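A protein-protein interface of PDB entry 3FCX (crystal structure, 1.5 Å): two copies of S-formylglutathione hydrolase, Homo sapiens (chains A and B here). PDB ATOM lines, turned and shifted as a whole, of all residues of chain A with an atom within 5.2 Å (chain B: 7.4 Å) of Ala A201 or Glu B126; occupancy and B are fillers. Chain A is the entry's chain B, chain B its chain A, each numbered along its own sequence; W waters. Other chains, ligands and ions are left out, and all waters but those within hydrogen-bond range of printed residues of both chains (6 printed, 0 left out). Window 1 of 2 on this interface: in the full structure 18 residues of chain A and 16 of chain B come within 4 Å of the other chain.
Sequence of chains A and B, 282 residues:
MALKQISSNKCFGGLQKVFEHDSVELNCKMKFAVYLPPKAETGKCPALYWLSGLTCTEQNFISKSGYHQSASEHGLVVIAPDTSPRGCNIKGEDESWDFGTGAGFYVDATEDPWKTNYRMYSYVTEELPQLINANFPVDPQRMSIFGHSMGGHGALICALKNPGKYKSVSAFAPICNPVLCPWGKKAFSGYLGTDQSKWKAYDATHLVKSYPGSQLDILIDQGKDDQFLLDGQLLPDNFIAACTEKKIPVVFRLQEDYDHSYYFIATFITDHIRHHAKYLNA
No position is printed for both chains.
N of Glu B127 touches OG of Ser A197, 3.9 Å away. Gln B130 touches Ser A197. Ala A201 touches Glu B126 (CB to OE2, 3.5 Å).
O of Ser A197 lies close to OE1 of Glu B126 (3.4 Å). The side-chain carboxylate of Glu B25 is in salt-bridge range of the side-chain amino group of Lys A198, at 3.2 Å.
The side-chain carboxylate (OE1) of Glu B127 lies within hydrogen-bond range of the backbone NH (N) of Glu B25 (3.0 Å). The backbone carbonyl oxygen (O) of Ser B122 lies within hydrogen-bond range of the backbone NH (N) of Glu B127 (3.1 Å). NZ of Lys A161 lies within hydrogen-bond range of O of Ala A201, at 2.8 Å.
Of the printed residues of chain B, Ser A197 touches Glu B126, Glu B127 and Gln B130. Of chain B, only Glu B126 comes within 4 Å of Ala A201. Asp A203 touches none of the printed residues of chain B. Tyr B123 touches none of the printed residues of chain A. Glu B126 touches just these residues of chain A: Ser A197 (3.4 Å) and Ala A201 (3.5 Å). Printed residues of chain A within 4 Å of Glu B127: Ser A197. The nearest residue of chain B that does not touch Ala A201 is Lys B165 (5.9 Å). The nearest printed residue of chain A that does not touch Glu B127 is Lys A198 (6.3 Å).
Water W5 lies within hydrogen-bond range of OE1 of Glu B126 (2.6 Å) and O of Ser A197 (2.7 Å). Water W3 lies within hydrogen-bond range of OD1 of Asn B162 (2.7 Å) and NZ of Lys A161 (3.2 Å). Water W2 bridges the side-chain amide nitrogen (NE2) of Gln B130 (2.7 Å) and the side-chain amino group (NZ) of Lys A200 (3.2 Å). Water W6 bridges the side-chain amino group (NZ) of Lys A198 (2.8 Å) and the side-chain carboxylate (OE1) of Glu B25 (3.2 Å). Water W1 bridges the side-chain amino group of Lys A161 (2.9 Å) and the side-chain carboxylate of Glu B126 (3.3 Å). Water W4 bridges O of Lys A198 (3.0 Å) and OE2 of Glu B126 (3.1 Å).
Hydrophobic or aromatic side chains of chain A that line the printed part of chain B: Ala A201. Along chain A the printed residues that touch a printed residue of chain B span positions 197 to 201. Among the printed residues, 5 pairs touch across the chains.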
ATOM      1  N   LYS A 161      27.199  -9.935  -5.273  1.00  0.00           N
ATOM      2  CA  LYS A 161      26.943 -11.199  -5.968  1.00  0.00           C
ATOM      3  C   LYS A 161      27.829 -12.335  -5.465  1.00  0.00           C
ATOM      4  O   LYS A 161      27.616 -13.502  -5.806  1.00  0.00           O
ATOM      5  CB  LYS A 161      27.138 -11.031  -7.475  1.00  0.00           C
ATOM      6  CG  LYS A 161      26.082 -10.171  -8.140  1.00  0.00           C
ATOM      7  CD  LYS A 161      26.450  -9.840  -9.585  1.00  0.00           C
ATOM      8  CE  LYS A 161      26.230 -11.027 -10.529  1.00  0.00           C
ATOM      9  NZ  LYS A 161      24.802 -11.425 -10.623  1.00  0.00           N
ATOM     10  N   SER A 197      15.132  -9.389 -16.040  1.00  0.00           N
ATOM     11  CA  SER A 197      15.516 -10.242 -14.922  1.00  0.00           C
ATOM     12  C   SER A 197      17.033 -10.386 -14.831  1.00  0.00           C
ATOM     13  O   SER A 197      17.608 -10.432 -13.759  1.00  0.00           O
ATOM     14  CB  SER A 197      14.863 -11.620 -15.047  1.00  0.00           C
ATOM     15  OG  SER A 197      15.328 -12.300 -16.199  1.00  0.00           O
ATOM     16  N   LYS A 198      17.594 -10.390 -15.999  1.00  0.00           N
ATOM     17  CA  LYS A 198      19.049 -10.363 -16.103  1.00  0.00           C
ATOM     18  C   LYS A 198      19.605  -9.056 -15.547  1.00  0.00           C
ATOM     19  O   LYS A 198      20.636  -9.061 -14.874  1.00  0.00           O
ATOM     20  CB  LYS A 198      19.488 -10.477 -17.562  1.00  0.00           C
ATOM     21  CG  LYS A 198      19.262 -11.811 -18.220  1.00  0.00           C
ATOM     22  CD  LYS A 198      19.136 -11.573 -19.707  1.00  0.00           C
ATOM     23  CE  LYS A 198      19.836 -12.636 -20.503  1.00  0.00           C
ATOM     24  NZ  LYS A 198      19.674 -12.382 -21.954  1.00  0.00           N
ATOM     25  N   TRP A 199      18.933  -7.946 -15.865  1.00  0.00           N
ATOM     26  CA  TRP A 199      19.392  -6.602 -15.496  1.00  0.00           C
ATOM     27  C   TRP A 199      19.477  -6.467 -13.984  1.00  0.00           C
ATOM     28  O   TRP A 199      20.451  -5.940 -13.458  1.00  0.00           O
ATOM     29  CB  TRP A 199      18.420  -5.527 -15.985  1.00  0.00           C
ATOM     30  CG  TRP A 199      18.267  -5.331 -17.466  1.00  0.00           C
ATOM     31  CD1 TRP A 199      18.539  -6.224 -18.464  1.00  0.00           C
ATOM     32  CD2 TRP A 199      17.736  -4.164 -18.103  1.00  0.00           C
ATOM     33  NE1 TRP A 199      18.233  -5.673 -19.688  1.00  0.00           N
ATOM     34  CE2 TRP A 199      17.736  -4.410 -19.495  1.00  0.00           C
ATOM     35  CE3 TRP A 199      17.271  -2.928 -17.631  1.00  0.00           C
ATOM     36  CZ2 TRP A 199      17.288  -3.462 -20.424  1.00  0.00           C
ATOM     37  CZ3 TRP A 199      16.828  -1.983 -18.555  1.00  0.00           C
ATOM     38  CH2 TRP A 199      16.839  -2.259 -19.938  1.00  0.00           C
ATOM     39  N   LYS A 200      18.438  -6.938 -13.296  1.00  0.00           N
ATOM     40  CA  LYS A 200      18.333  -6.805 -11.846  1.00  0.00           C
ATOM     41  C   LYS A 200      19.467  -7.519 -11.114  1.00  0.00           C
ATOM     42  O   LYS A 200      19.869  -7.104 -10.027  1.00  0.00           O
ATOM     43  CB  LYS A 200      16.968  -7.308 -11.360  1.00  0.00           C
ATOM     44  CG  LYS A 200      15.807  -6.415 -11.769  1.00  0.00           C
ATOM     45  CD  LYS A 200      14.464  -7.056 -11.442  1.00  0.00           C
ATOM     46  CE  LYS A 200      13.320  -6.048 -11.530  1.00  0.00           C
ATOM     47  NZ  LYS A 200      13.136  -5.469 -12.895  1.00  0.00           N
ATOM     48  N   ALA A 201      19.984  -8.584 -11.720  1.00  0.00           N
ATOM     49  CA  ALA A 201      21.102  -9.338 -11.154  1.00  0.00           C
ATOM     50  C   ALA A 201      22.428  -8.574 -11.243  1.00  0.00           C
ATOM     51  O   ALA A 201      23.452  -9.029 -10.726  1.00  0.00           O
ATOM     52  CB  ALA A 201      21.217 -10.697 -11.825  1.00  0.00           C
ATOM     53  N   TYR A 202      22.401  -7.418 -11.903  1.00  0.00           N
ATOM     54  CA  TYR A 202      23.583  -6.568 -12.035  1.00  0.00           C
ATOM     55  C   TYR A 202      23.311  -5.149 -11.516  1.00  0.00           C
ATOM     56  O   TYR A 202      23.974  -4.192 -11.923  1.00  0.00           O
ATOM     57  CB  TYR A 202      24.034  -6.502 -13.496  1.00  0.00           C
ATOM     58  CG  TYR A 202      24.712  -7.748 -14.038  1.00  0.00           C
ATOM     59  CD1 TYR A 202      26.037  -8.044 -13.713  1.00  0.00           C
ATOM     60  CD2 TYR A 202      24.042  -8.606 -14.909  1.00  0.00           C
ATOM     61  CE1 TYR A 202      26.670  -9.183 -14.221  1.00  0.00           C
ATOM     62  CE2 TYR A 202      24.664  -9.742 -15.425  1.00  0.00           C
ATOM     63  CZ  TYR A 202      25.976 -10.025 -15.085  1.00  0.00           C
ATOM     64  OH  TYR A 202      26.594 -11.146 -15.610  1.00  0.00           O
ATOM     65  N   ASP A 203      22.338  -5.022 -10.613  1.00  0.00           N
ATOM     66  CA  ASP A 203      21.937  -3.727 -10.081  1.00  0.00           C
ATOM     67  C   ASP A 203      22.140  -3.741  -8.567  1.00  0.00           C
ATOM     68  O   ASP A 203      21.519  -4.541  -7.874  1.00  0.00           O
ATOM     69  CB  ASP A 203      20.471  -3.457 -10.457  1.00  0.00           C
ATOM     70  CG  ASP A 203      19.962  -2.124  -9.948  1.00  0.00           C
ATOM     71  OD1 ASP A 203      20.041  -1.867  -8.729  1.00  0.00           O
ATOM     72  OD2 ASP A 203      19.448  -1.334 -10.767  1.00  0.00           O
ATOM     73  N   LEU A 207      20.343  -5.991  -5.759  1.00  0.00           N
ATOM     74  CA  LEU A 207      21.184  -7.037  -5.174  1.00  0.00           C
ATOM     75  C   LEU A 207      21.269  -6.965  -3.656  1.00  0.00           C
ATOM     76  O   LEU A 207      21.268  -7.996  -2.984  1.00  0.00           O
ATOM     77  CB  LEU A 207      22.588  -7.018  -5.786  1.00  0.00           C
ATOM     78  CG  LEU A 207      22.658  -7.583  -7.208  1.00  0.00           C
ATOM     79  CD1 LEU A 207      23.944  -7.148  -7.877  1.00  0.00           C
ATOM     80  CD2 LEU A 207      22.535  -9.107  -7.210  1.00  0.00           C
ATOM     81  N   GLU B  25      13.708 -15.983 -22.707  1.00  0.00           N
ATOM     82  CA  GLU B  25      15.062 -16.486 -22.944  1.00  0.00           C
ATOM     83  C   GLU B  25      15.116 -17.515 -24.063  1.00  0.00           C
ATOM     84  O   GLU B  25      16.070 -17.545 -24.850  1.00  0.00           O
ATOM     85  CB  GLU B  25      15.657 -17.093 -21.670  1.00  0.00           C
ATOM     86  CG  GLU B  25      16.059 -16.072 -20.619  1.00  0.00           C
ATOM     87  CD  GLU B  25      17.170 -15.146 -21.084  1.00  0.00           C
ATOM     88  OE1 GLU B  25      18.048 -15.575 -21.862  1.00  0.00           O
ATOM     89  OE2 GLU B  25      17.168 -13.976 -20.662  1.00  0.00           O
ATOM     90  N   MET B 120      19.437 -22.036 -21.656  1.00  0.00           N
ATOM     91  CA  MET B 120      18.964 -22.745 -20.468  1.00  0.00           C
ATOM     92  C   MET B 120      19.586 -22.278 -19.159  1.00  0.00           C
ATOM     93  O   MET B 120      18.924 -22.321 -18.121  1.00  0.00           O
ATOM     94  CB  MET B 120      19.103 -24.260 -20.643  1.00  0.00           C
ATOM     95  CG  MET B 120      18.075 -24.865 -21.605  1.00  0.00           C
ATOM     96  SD  MET B 120      16.350 -24.632 -21.099  1.00  0.00           S
ATOM     97  CE  MET B 120      16.296 -25.549 -19.558  1.00  0.00           C
ATOM     98  N   TYR B 121      20.837 -21.826 -19.197  1.00  0.00           N
ATOM     99  CA  TYR B 121      21.468 -21.292 -17.989  1.00  0.00           C
ATOM    100  C   TYR B 121      20.726 -20.045 -17.503  1.00  0.00           C
ATOM    101  O   TYR B 121      20.359 -19.953 -16.331  1.00  0.00           O
ATOM    102  CB  TYR B 121      22.958 -20.997 -18.208  1.00  0.00           C
ATOM    103  CG  TYR B 121      23.605 -20.308 -17.028  1.00  0.00           C
ATOM    104  CD1 TYR B 121      23.895 -21.013 -15.862  1.00  0.00           C
ATOM    105  CD2 TYR B 121      23.903 -18.947 -17.070  1.00  0.00           C
ATOM    106  CE1 TYR B 121      24.476 -20.384 -14.770  1.00  0.00           C
ATOM    107  CE2 TYR B 121      24.482 -18.308 -15.983  1.00  0.00           C
ATOM    108  CZ  TYR B 121      24.764 -19.033 -14.835  1.00  0.00           C
ATOM    109  OH  TYR B 121      25.343 -18.409 -13.753  1.00  0.00           O
ATOM    110  N   SER B 122      20.491 -19.095 -18.404  1.00  0.00           N
ATOM    111  CA  SER B 122      19.754 -17.882 -18.053  1.00  0.00           C
ATOM    112  C   SER B 122      18.295 -18.176 -17.698  1.00  0.00           C
ATOM    113  O   SER B 122      17.723 -17.510 -16.834  1.00  0.00           O
ATOM    114  CB  SER B 122      19.809 -16.859 -19.191  1.00  0.00           C
ATOM    115  OG  SER B 122      21.102 -16.296 -19.308  1.00  0.00           O
ATOM    116  N   TYR B 123      17.694 -19.163 -18.366  1.00  0.00           N
ATOM    117  CA  TYR B 123      16.320 -19.561 -18.057  1.00  0.00           C
ATOM    118  C   TYR B 123      16.200 -20.066 -16.617  1.00  0.00           C
ATOM    119  O   TYR B 123      15.338 -19.603 -15.864  1.00  0.00           O
ATOM    120  CB  TYR B 123      15.818 -20.628 -19.037  1.00  0.00           C
ATOM    121  CG  TYR B 123      14.389 -21.060 -18.792  1.00  0.00           C
ATOM    122  CD1 TYR B 123      13.323 -20.208 -19.082  1.00  0.00           C
ATOM    123  CD2 TYR B 123      14.102 -22.324 -18.274  1.00  0.00           C
ATOM    124  CE1 TYR B 123      12.007 -20.603 -18.857  1.00  0.00           C
ATOM    125  CE2 TYR B 123      12.788 -22.733 -18.051  1.00  0.00           C
ATOM    126  CZ  TYR B 123      11.747 -21.866 -18.344  1.00  0.00           C
ATOM    127  OH  TYR B 123      10.452 -22.263 -18.125  1.00  0.00           O
ATOM    128  N   VAL B 124      17.042 -21.041 -16.285  1.00  0.00           N
ATOM    129  CA  VAL B 124      17.027 -21.613 -14.948  1.00  0.00           C
ATOM    130  C   VAL B 124      17.388 -20.616 -13.795  1.00  0.00           C
ATOM    131  O   VAL B 124      16.754 -20.627 -12.757  1.00  0.00           O
ATOM    132  CB  VAL B 124      17.980 -22.838 -14.824  1.00  0.00           C
ATOM    133  CG1 VAL B 124      18.077 -23.243 -13.319  1.00  0.00           C
ATOM    134  CG2 VAL B 124      17.453 -23.951 -15.693  1.00  0.00           C
ATOM    135  N   THR B 125      18.397 -19.785 -14.030  1.00  0.00           N
ATOM    136  CA  THR B 125      18.924 -18.907 -12.976  1.00  0.00           C
ATOM    137  C   THR B 125      18.227 -17.553 -12.874  1.00  0.00           C
ATOM    138  O   THR B 125      18.219 -16.950 -11.799  1.00  0.00           O
ATOM    139  CB  THR B 125      20.445 -18.669 -13.109  1.00  0.00           C
ATOM    140  OG1 THR B 125      20.730 -18.056 -14.370  1.00  0.00           O
ATOM    141  CG2 THR B 125      21.214 -19.978 -12.983  1.00  0.00           C
ATOM    142  N   GLU B 126      17.649 -17.076 -13.976  1.00  0.00           N
ATOM    143  CA  GLU B 126      17.052 -15.737 -13.991  1.00  0.00           C
ATOM    144  C   GLU B 126      15.561 -15.716 -14.356  1.00  0.00           C
ATOM    145  O   GLU B 126      14.735 -15.267 -13.550  1.00  0.00           O
ATOM    146  CB  GLU B 126      17.846 -14.774 -14.895  1.00  0.00           C
ATOM    147  CG  GLU B 126      19.364 -14.693 -14.627  1.00  0.00           C
ATOM    148  CD  GLU B 126      19.735 -13.942 -13.350  1.00  0.00           C
ATOM    149  OE1 GLU B 126      18.840 -13.366 -12.694  1.00  0.00           O
ATOM    150  OE2 GLU B 126      20.939 -13.929 -13.003  1.00  0.00           O
ATOM    151  N   GLU B 127      15.209 -16.187 -15.554  1.00  0.00           N
ATOM    152  CA  GLU B 127      13.827 -16.054 -16.019  1.00  0.00           C
ATOM    153  C   GLU B 127      12.836 -16.869 -15.192  1.00  0.00           C
ATOM    154  O   GLU B 127      11.826 -16.335 -14.727  1.00  0.00           O
ATOM    155  CB  GLU B 127      13.666 -16.385 -17.509  1.00  0.00           C
ATOM    156  CG  GLU B 127      12.284 -15.963 -18.007  1.00  0.00           C
ATOM    157  CD  GLU B 127      11.924 -16.446 -19.398  1.00  0.00           C
ATOM    158  OE1 GLU B 127      12.752 -17.097 -20.060  1.00  0.00           O
ATOM    159  OE2 GLU B 127      10.784 -16.164 -19.819  1.00  0.00           O
ATOM    160  N   LEU B 128      13.123 -18.155 -15.011  1.00  0.00           N
ATOM    161  CA  LEU B 128      12.190 -19.037 -14.312  1.00  0.00           C
ATOM    162  C   LEU B 128      11.915 -18.606 -12.866  1.00  0.00           C
ATOM    163  O   LEU B 128      10.746 -18.518 -12.480  1.00  0.00           O
ATOM    164  CB  LEU B 128      12.622 -20.505 -14.399  1.00  0.00           C
ATOM    165  CG  LEU B 128      11.665 -21.536 -13.797  1.00  0.00           C
ATOM    166  CD1 LEU B 128      10.300 -21.502 -14.476  1.00  0.00           C
ATOM    167  CD2 LEU B 128      12.280 -22.927 -13.882  1.00  0.00           C
ATOM    168  N   PRO B 129      12.970 -18.317 -12.069  1.00  0.00           N
ATOM    169  CA  PRO B 129      12.689 -17.859 -10.705  1.00  0.00           C
ATOM    170  C   PRO B 129      11.863 -16.576 -10.655  1.00  0.00           C
ATOM    171  O   PRO B 129      11.005 -16.450  -9.787  1.00  0.00           O
ATOM    172  CB  PRO B 129      14.083 -17.634 -10.111  1.00  0.00           C
ATOM    173  CG  PRO B 129      14.949 -18.572 -10.863  1.00  0.00           C
ATOM    174  CD  PRO B 129      14.413 -18.550 -12.268  1.00  0.00           C
ATOM    175  N   GLN B 130      12.095 -15.649 -11.586  1.00  0.00           N
ATOM    176  CA  GLN B 130      11.276 -14.432 -11.668  1.00  0.00           C
ATOM    177  C   GLN B 130       9.801 -14.789 -11.889  1.00  0.00           C
ATOM    178  O   GLN B 130       8.905 -14.226 -11.251  1.00  0.00           O
ATOM    179  CB  GLN B 130      11.773 -13.499 -12.780  1.00  0.00           C
ATOM    180  CG  GLN B 130      10.969 -12.206 -12.903  1.00  0.00           C
ATOM    181  CD  GLN B 130      11.385 -11.352 -14.085  1.00  0.00           C
ATOM    182  OE1 GLN B 130      11.221 -11.744 -15.244  1.00  0.00           O
ATOM    183  NE2 GLN B 130      11.914 -10.166 -13.795  1.00  0.00           N
ATOM    184  N   LEU B 131       9.561 -15.739 -12.785  1.00  0.00           N
ATOM    185  CA  LEU B 131       8.210 -16.173 -13.112  1.00  0.00           C
ATOM    186  C   LEU B 131       7.538 -16.867 -11.927  1.00  0.00           C
ATOM    187  O   LEU B 131       6.375 -16.598 -11.610  1.00  0.00           O
ATOM    188  CB  LEU B 131       8.244 -17.096 -14.331  1.00  0.00           C
ATOM    189  CG  LEU B 131       6.901 -17.538 -14.902  1.00  0.00           C
ATOM    190  CD1 LEU B 131       6.223 -16.396 -15.662  1.00  0.00           C
ATOM    191  CD2 LEU B 131       7.128 -18.729 -15.806  1.00  0.00           C
ATOM    192  N   ILE B 132       8.277 -17.759 -11.275  1.00  0.00           N
ATOM    193  CA  ILE B 132       7.770 -18.467 -10.103  1.00  0.00           C
ATOM    194  C   ILE B 132       7.408 -17.489  -8.987  1.00  0.00           C
ATOM    195  O   ILE B 132       6.330 -17.586  -8.395  1.00  0.00           O
ATOM    196  CB  ILE B 132       8.787 -19.528  -9.602  1.00  0.00           C
ATOM    197  CG1 ILE B 132       9.017 -20.613 -10.674  1.00  0.00           C
ATOM    198  CG2 ILE B 132       8.354 -20.121  -8.259  1.00  0.00           C
ATOM    199  CD1 ILE B 132       7.768 -21.353 -11.140  1.00  0.00           C
ATOM    200  N   ASN B 133       8.303 -16.541  -8.717  1.00  0.00           N
ATOM    201  CA  ASN B 133       8.093 -15.581  -7.637  1.00  0.00           C
ATOM    202  C   ASN B 133       6.884 -14.683  -7.872  1.00  0.00           C
ATOM    203  O   ASN B 133       6.207 -14.291  -6.921  1.00  0.00           O
ATOM    204  CB  ASN B 133       9.356 -14.747  -7.411  1.00  0.00           C
ATOM    205  CG  ASN B 133      10.523 -15.586  -6.914  1.00  0.00           C
ATOM    206  OD1 ASN B 133      10.337 -16.697  -6.406  1.00  0.00           O
ATOM    207  ND2 ASN B 133      11.733 -15.058  -7.057  1.00  0.00           N
ATOM    208  N   MET B 143      15.929 -20.182  -1.997  1.00  0.00           N
ATOM    209  CA  MET B 143      15.909 -21.026  -3.176  1.00  0.00           C
ATOM    210  C   MET B 143      17.082 -21.999  -3.100  1.00  0.00           C
ATOM    211  O   MET B 143      18.195 -21.610  -2.722  1.00  0.00           O
ATOM    212  CB  MET B 143      16.007 -20.140  -4.427  1.00  0.00           C
ATOM    213  CG  MET B 143      16.213 -20.847  -5.739  1.00  0.00           C
ATOM    214  SD  MET B 143      16.016 -19.696  -7.114  1.00  0.00           S
ATOM    215  CE  MET B 143      17.455 -18.643  -6.931  1.00  0.00           C
ATOM    216  N   ASN B 162      26.971 -18.817  -8.862  1.00  0.00           N
ATOM    217  CA  ASN B 162      26.165 -17.792  -8.214  1.00  0.00           C
ATOM    218  C   ASN B 162      26.209 -17.948  -6.696  1.00  0.00           C
ATOM    219  O   ASN B 162      25.218 -18.379  -6.096  1.00  0.00           O
ATOM    220  CB  ASN B 162      24.724 -17.877  -8.720  1.00  0.00           C
ATOM    221  CG  ASN B 162      24.614 -17.638 -10.214  1.00  0.00           C
ATOM    222  OD1 ASN B 162      24.595 -16.494 -10.663  1.00  0.00           O
ATOM    223  ND2 ASN B 162      24.523 -18.719 -10.990  1.00  0.00           N
ATOM    224  N   LYS B 165      23.335 -17.557  -3.930  1.00  0.00           N
ATOM    225  CA  LYS B 165      22.042 -17.489  -4.626  1.00  0.00           C
ATOM    226  C   LYS B 165      21.156 -18.665  -4.223  1.00  0.00           C
ATOM    227  O   LYS B 165      19.931 -18.532  -4.090  1.00  0.00           O
ATOM    228  CB  LYS B 165      22.253 -17.503  -6.141  1.00  0.00           C
ATOM    229  CG  LYS B 165      20.995 -17.264  -6.966  1.00  0.00           C
ATOM    230  CD  LYS B 165      21.286 -17.424  -8.452  1.00  0.00           C
ATOM    231  CE  LYS B 165      20.044 -17.222  -9.294  1.00  0.00           C
ATOM    232  NZ  LYS B 165      19.653 -15.789  -9.397  1.00  0.00           N
ATOM    233  N   TYR B 166      21.794 -19.815  -4.036  1.00  0.00           N
ATOM    234  CA  TYR B 166      21.123 -21.024  -3.591  1.00  0.00           C
ATOM    235  C   TYR B 166      21.585 -21.368  -2.184  1.00  0.00           C
ATOM    236  O   TYR B 166      22.778 -21.281  -1.877  1.00  0.00           O
ATOM    237  CB  TYR B 166      21.414 -22.173  -4.556  1.00  0.00           C
ATOM    238  CG  TYR B 166      20.918 -21.891  -5.956  1.00  0.00           C
ATOM    239  CD1 TYR B 166      19.587 -22.122  -6.303  1.00  0.00           C
ATOM    240  CD2 TYR B 166      21.769 -21.358  -6.924  1.00  0.00           C
ATOM    241  CE1 TYR B 166      19.122 -21.851  -7.587  1.00  0.00           C
ATOM    242  CE2 TYR B 166      21.312 -21.079  -8.210  1.00  0.00           C
ATOM    243  CZ  TYR B 166      19.991 -21.329  -8.533  1.00  0.00           C
ATOM    244  OH  TYR B 166      19.526 -21.062  -9.801  1.00  0.00           O
HETATM  245  O   HOH W   1      24.014 -12.833 -12.984  1.00  0.00           O
HETATM  246  O   HOH W   2      11.958  -7.655 -14.865  1.00  0.00           O
HETATM  247  O   HOH W   3      25.431 -14.311  -9.396  1.00  0.00           O
HETATM  248  O   HOH W   4      22.005 -11.715 -14.857  1.00  0.00           O
HETATM  249  O   HOH W   5      17.188 -11.758 -11.400  1.00  0.00           O
HETATM  250  O   HOH W   6      18.753 -13.549 -24.303  1.00  0.00           O
